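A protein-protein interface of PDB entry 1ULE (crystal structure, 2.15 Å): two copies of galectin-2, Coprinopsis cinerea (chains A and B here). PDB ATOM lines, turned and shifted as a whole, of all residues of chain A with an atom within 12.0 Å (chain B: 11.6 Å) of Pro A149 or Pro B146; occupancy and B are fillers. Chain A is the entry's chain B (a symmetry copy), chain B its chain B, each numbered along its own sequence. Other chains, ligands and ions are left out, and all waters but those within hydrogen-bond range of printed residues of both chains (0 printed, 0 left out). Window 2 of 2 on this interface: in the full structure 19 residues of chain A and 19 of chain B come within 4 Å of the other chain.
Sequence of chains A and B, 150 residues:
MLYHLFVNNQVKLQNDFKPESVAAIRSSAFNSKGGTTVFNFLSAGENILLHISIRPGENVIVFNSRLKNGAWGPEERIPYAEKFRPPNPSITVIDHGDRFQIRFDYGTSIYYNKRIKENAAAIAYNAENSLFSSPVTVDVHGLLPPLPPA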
ATOM      1  N   PRO A 145      20.671 -24.295  -4.754  1.00  0.00           N
ATOM      2  CA  PRO A 145      19.552 -24.503  -3.827  1.00  0.00           C
ATOM      3  C   PRO A 145      18.273 -24.889  -4.570  1.00  0.00           C
ATOM      4  O   PRO A 145      18.209 -24.796  -5.797  1.00  0.00           O
ATOM      5  CB  PRO A 145      19.419 -23.146  -3.153  1.00  0.00           C
ATOM      6  CG  PRO A 145      19.708 -22.208  -4.297  1.00  0.00           C
ATOM      7  CD  PRO A 145      20.914 -22.856  -4.970  1.00  0.00           C
ATOM      8  N   PRO A 146      17.240 -25.336  -3.836  1.00  0.00           N
ATOM      9  CA  PRO A 146      15.979 -25.716  -4.483  1.00  0.00           C
ATOM     10  C   PRO A 146      15.447 -24.493  -5.220  1.00  0.00           C
ATOM     11  O   PRO A 146      15.584 -23.367  -4.737  1.00  0.00           O
ATOM     12  CB  PRO A 146      15.098 -26.119  -3.306  1.00  0.00           C
ATOM     13  CG  PRO A 146      16.104 -26.661  -2.311  1.00  0.00           C
ATOM     14  CD  PRO A 146      17.196 -25.622  -2.390  1.00  0.00           C
ATOM     15  N   LEU A 147      14.841 -24.710  -6.379  1.00  0.00           N
ATOM     16  CA  LEU A 147      14.331 -23.609  -7.183  1.00  0.00           C
ATOM     17  C   LEU A 147      12.830 -23.346  -7.071  1.00  0.00           C
ATOM     18  O   LEU A 147      12.020 -24.273  -7.020  1.00  0.00           O
ATOM     19  CB  LEU A 147      14.673 -23.851  -8.654  1.00  0.00           C
ATOM     20  CG  LEU A 147      16.138 -24.129  -8.992  1.00  0.00           C
ATOM     21  CD1 LEU A 147      16.256 -24.414 -10.482  1.00  0.00           C
ATOM     22  CD2 LEU A 147      17.007 -22.934  -8.588  1.00  0.00           C
ATOM     23  N   PRO A 148      12.441 -22.063  -7.028  1.00  0.00           N
ATOM     24  CA  PRO A 148      11.017 -21.742  -6.933  1.00  0.00           C
ATOM     25  C   PRO A 148      10.399 -22.103  -8.280  1.00  0.00           C
ATOM     26  O   PRO A 148      11.097 -22.144  -9.294  1.00  0.00           O
ATOM     27  CB  PRO A 148      11.022 -20.238  -6.670  1.00  0.00           C
ATOM     28  CG  PRO A 148      12.245 -19.781  -7.405  1.00  0.00           C
ATOM     29  CD  PRO A 148      13.257 -20.837  -7.023  1.00  0.00           C
ATOM     30  N   PRO A 149       9.086 -22.370  -8.309  1.00  0.00           N
ATOM     31  CA  PRO A 149       8.412 -22.730  -9.561  1.00  0.00           C
ATOM     32  C   PRO A 149       8.614 -21.697 -10.660  1.00  0.00           C
ATOM     33  O   PRO A 149       8.524 -22.011 -11.845  1.00  0.00           O
ATOM     34  CB  PRO A 149       6.952 -22.863  -9.140  1.00  0.00           C
ATOM     35  CG  PRO A 149       6.840 -21.892  -8.005  1.00  0.00           C
ATOM     36  CD  PRO A 149       8.105 -22.166  -7.229  1.00  0.00           C
ATOM     37  N   ALA A 150       8.892 -20.463 -10.258  1.00  0.00           N
ATOM     38  CA  ALA A 150       9.111 -19.387 -11.213  1.00  0.00           C
ATOM     39  C   ALA A 150      10.350 -18.584 -10.826  1.00  0.00           C
ATOM     40  O   ALA A 150      11.240 -18.427 -11.690  1.00  0.00           O
ATOM     41  CB  ALA A 150       7.882 -18.476 -11.270  1.00  0.00           C
ATOM     42  OXT ALA A 150      10.418 -18.120  -9.667  1.00  0.00           O
ATOM     43  N   GLU B  20      -0.042  -6.789   1.378  1.00  0.00           N
ATOM     44  CA  GLU B  20       0.535  -7.806   0.492  1.00  0.00           C
ATOM     45  C   GLU B  20       2.052  -7.657   0.394  1.00  0.00           C
ATOM     46  O   GLU B  20       2.752  -8.622   0.081  1.00  0.00           O
ATOM     47  CB  GLU B  20      -0.064  -7.747  -0.920  1.00  0.00           C
ATOM     48  CG  GLU B  20      -1.551  -8.058  -1.017  1.00  0.00           C
ATOM     49  CD  GLU B  20      -1.903  -9.442  -0.504  1.00  0.00           C
ATOM     50  OE1 GLU B  20      -1.236 -10.423  -0.895  1.00  0.00           O
ATOM     51  OE2 GLU B  20      -2.863  -9.553   0.283  1.00  0.00           O
ATOM     52  N   VAL B  22       6.020  -7.425   1.181  1.00  0.00           N
ATOM     53  CA  VAL B  22       6.904  -8.230   2.016  1.00  0.00           C
ATOM     54  C   VAL B  22       8.297  -7.609   2.024  1.00  0.00           C
ATOM     55  O   VAL B  22       8.850  -7.314   0.965  1.00  0.00           O
ATOM     56  CB  VAL B  22       7.036  -9.665   1.469  1.00  0.00           C
ATOM     57  CG1 VAL B  22       7.979 -10.477   2.367  1.00  0.00           C
ATOM     58  CG2 VAL B  22       5.661 -10.328   1.377  1.00  0.00           C
ATOM     59  N   VAL B 140      12.392  -5.926  -1.007  1.00  0.00           N
ATOM     60  CA  VAL B 140      10.984  -5.589  -0.821  1.00  0.00           C
ATOM     61  C   VAL B 140      10.138  -6.096  -1.986  1.00  0.00           C
ATOM     62  O   VAL B 140      10.426  -5.805  -3.147  1.00  0.00           O
ATOM     63  CB  VAL B 140      10.784  -4.063  -0.690  1.00  0.00           C
ATOM     64  CG1 VAL B 140       9.310  -3.753  -0.436  1.00  0.00           C
ATOM     65  CG2 VAL B 140      11.645  -3.516   0.449  1.00  0.00           C
ATOM     66  N   HIS B 141       9.087  -6.844  -1.657  1.00  0.00           N
ATOM     67  CA  HIS B 141       8.181  -7.426  -2.643  1.00  0.00           C
ATOM     68  C   HIS B 141       6.791  -6.781  -2.572  1.00  0.00           C
ATOM     69  O   HIS B 141       6.328  -6.404  -1.491  1.00  0.00           O
ATOM     70  CB  HIS B 141       8.004  -8.927  -2.373  1.00  0.00           C
ATOM     71  CG  HIS B 141       9.287  -9.697  -2.291  1.00  0.00           C
ATOM     72  ND1 HIS B 141       9.839 -10.343  -3.376  1.00  0.00           N
ATOM     73  CD2 HIS B 141      10.115  -9.942  -1.247  1.00  0.00           C
ATOM     74  CE1 HIS B 141      10.951 -10.955  -3.004  1.00  0.00           C
ATOM     75  NE2 HIS B 141      11.141 -10.728  -1.717  1.00  0.00           N
ATOM     76  N   GLY B 142       6.126  -6.684  -3.721  1.00  0.00           N
ATOM     77  CA  GLY B 142       4.784  -6.128  -3.768  1.00  0.00           C
ATOM     78  C   GLY B 142       3.765  -7.196  -3.385  1.00  0.00           C
ATOM     79  O   GLY B 142       2.611  -6.899  -3.074  1.00  0.00           O
ATOM     80  N   LEU B 143       4.199  -8.453  -3.419  1.00  0.00           N
ATOM     81  CA  LEU B 143       3.361  -9.589  -3.052  1.00  0.00           C
ATOM     82  C   LEU B 143       4.276 -10.785  -2.821  1.00  0.00           C
ATOM     83  O   LEU B 143       5.411 -10.799  -3.289  1.00  0.00           O
ATOM     84  CB  LEU B 143       2.350  -9.912  -4.157  1.00  0.00           C
ATOM     85  CG  LEU B 143       2.824 -10.653  -5.407  1.00  0.00           C
ATOM     86  CD1 LEU B 143       1.634 -10.852  -6.336  1.00  0.00           C
ATOM     87  CD2 LEU B 143       3.922  -9.871  -6.102  1.00  0.00           C
ATOM     88  N   LEU B 144       3.792 -11.779  -2.085  1.00  0.00           N
ATOM     89  CA  LEU B 144       4.593 -12.960  -1.806  1.00  0.00           C
ATOM     90  C   LEU B 144       4.974 -13.617  -3.134  1.00  0.00           C
ATOM     91  O   LEU B 144       4.110 -13.907  -3.958  1.00  0.00           O
ATOM     92  CB  LEU B 144       3.797 -13.945  -0.947  1.00  0.00           C
ATOM     93  CG  LEU B 144       4.575 -15.067  -0.256  1.00  0.00           C
ATOM     94  CD1 LEU B 144       5.511 -14.478   0.795  1.00  0.00           C
ATOM     95  CD2 LEU B 144       3.591 -16.030   0.394  1.00  0.00           C
ATOM     96  N   PRO B 145       6.276 -13.851  -3.359  1.00  0.00           N
ATOM     97  CA  PRO B 145       6.758 -14.480  -4.596  1.00  0.00           C
ATOM     98  C   PRO B 145       6.587 -15.998  -4.555  1.00  0.00           C
ATOM     99  O   PRO B 145       6.289 -16.568  -3.505  1.00  0.00           O
ATOM    100  CB  PRO B 145       8.226 -14.083  -4.622  1.00  0.00           C
ATOM    101  CG  PRO B 145       8.590 -14.163  -3.163  1.00  0.00           C
ATOM    102  CD  PRO B 145       7.404 -13.490  -2.479  1.00  0.00           C
ATOM    103  N   PRO B 146       6.766 -16.673  -5.704  1.00  0.00           N
ATOM    104  CA  PRO B 146       6.626 -18.133  -5.735  1.00  0.00           C
ATOM    105  C   PRO B 146       7.643 -18.720  -4.765  1.00  0.00           C
ATOM    106  O   PRO B 146       8.755 -18.204  -4.641  1.00  0.00           O
ATOM    107  CB  PRO B 146       6.940 -18.476  -7.188  1.00  0.00           C
ATOM    108  CG  PRO B 146       6.458 -17.245  -7.928  1.00  0.00           C
ATOM    109  CD  PRO B 146       7.000 -16.137  -7.057  1.00  0.00           C
ATOM    110  N   LEU B 147       7.267 -19.793  -4.081  1.00  0.00           N
ATOM    111  CA  LEU B 147       8.147 -20.409  -3.098  1.00  0.00           C
ATOM    112  C   LEU B 147       8.904 -21.649  -3.571  1.00  0.00           C
ATOM    113  O   LEU B 147       8.360 -22.500  -4.277  1.00  0.00           O
ATOM    114  CB  LEU B 147       7.340 -20.778  -1.853  1.00  0.00           C
ATOM    115  CG  LEU B 147       6.505 -19.670  -1.208  1.00  0.00           C
ATOM    116  CD1 LEU B 147       5.727 -20.253  -0.038  1.00  0.00           C
ATOM    117  CD2 LEU B 147       7.417 -18.526  -0.748  1.00  0.00           C
ATOM    118  N   PRO B 148      10.182 -21.763  -3.182  1.00  0.00           N
ATOM    119  CA  PRO B 148      10.960 -22.932  -3.590  1.00  0.00           C
ATOM    120  C   PRO B 148      10.400 -24.120  -2.815  1.00  0.00           C
ATOM    121  O   PRO B 148       9.804 -23.944  -1.751  1.00  0.00           O
ATOM    122  CB  PRO B 148      12.379 -22.566  -3.163  1.00  0.00           C
ATOM    123  CG  PRO B 148      12.147 -21.721  -1.948  1.00  0.00           C
ATOM    124  CD  PRO B 148      11.007 -20.833  -2.392  1.00  0.00           C
ATOM    125  N   PRO B 149      10.579 -25.342  -3.336  1.00  0.00           N
ATOM    126  CA  PRO B 149      10.068 -26.538  -2.658  1.00  0.00           C
ATOM    127  C   PRO B 149      10.560 -26.661  -1.223  1.00  0.00           C
ATOM    128  O   PRO B 149       9.922 -27.302  -0.390  1.00  0.00           O
ATOM    129  CB  PRO B 149      10.562 -27.675  -3.548  1.00  0.00           C
ATOM    130  CG  PRO B 149      11.831 -27.125  -4.121  1.00  0.00           C
ATOM    131  CD  PRO B 149      11.432 -25.714  -4.478  1.00  0.00           C
ATOM    132  N   ALA B 150      11.696 -26.037  -0.938  1.00  0.00           N
ATOM    133  CA  ALA B 150      12.266 -26.075   0.399  1.00  0.00           C
ATOM    134  C   ALA B 150      12.703 -24.676   0.826  1.00  0.00           C
ATOM    135  O   ALA B 150      12.272 -24.232   1.911  1.00  0.00           O
ATOM    136  CB  ALA B 150      13.455 -27.039   0.437  1.00  0.00           C
ATOM    137  OXT ALA B 150      13.474 -24.040   0.071  1.00  0.00           O
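O of Pro A146 touches CB of Pro B148 (3.7 Å). Pro B149 touches Pro A146 (CG to CB, 3.5 Å). CB of Ala B150 touches CG of Pro A146, at 3.8 Å. O of Leu A147 touches CD of Pro B149 (3.0 Å). Pro B146 touches Pro A148. O of Leu B147 touches CA of Pro A148 (3.8 Å). Pro A148 touches Pro B148 (CA to CA, 3.5 Å). CG of Pro A149 touches CB of Pro B146, at 3.5 Å. Pro A149 touches Leu B147. CB of Ala A150 touches CG of Pro B146 (3.8 Å).
Pro A145 touches none of the printed residues of chain B. Of chain B, only Pro B146 (3.7 Å), Leu B147 (3.8 Å) and Pro B148 (3.5 Å) come within 4 Å of Pro A148. Ala A150 touches one residue of chain B. Leu B143 touches none of the printed residues of chain A. No residue of chain A comes within 4 Å of Pro B145. Of chain A, only Pro A148 and Pro A149 come within 4 Å of Leu B147. Pro B148 touches just these residues of chain A: Pro A146 (3.7 Å), Leu A147 (3.8 Å) and Pro A148 (3.5 Å). Of the printed residues of chain A, Pro B149 touches Pro A146 and Leu A147. Of the printed residues of chain A, Ala B150 touches Pro A146. The nearest residue of chain B that does not touch Pro A149 is Pro B148 (4.6 Å).
Printed residues of chain A that touch a printed residue of chain B: Pro A146, Leu A147, Pro A148, Pro A149 and Ala A150. Hydrophobic or aromatic side chains of chain A within 4 Å of the printed part of chain B: Pro A146, Pro A148, Pro A149 and Ala A150. Among the printed residues, no Asp or Glu carboxylate lies within 4 Å of a Lys or Arg side-chain nitrogen of the other chain.
Pro A146 touches Pro B148, and with the chains exchanged Pro A148 touches Pro B146. Leu A147 touches Pro B148, and with the chains exchanged Pro A148 touches Leu B147. Leu A147 touches Pro B149, and with the chains exchanged Pro A149 touches Leu B147. Pro B148 touches its own counterpart, Pro A148. Of the 11 pairs that touch across the chains among the printed residues, 11 have their exchanged pair printed and touching as well.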
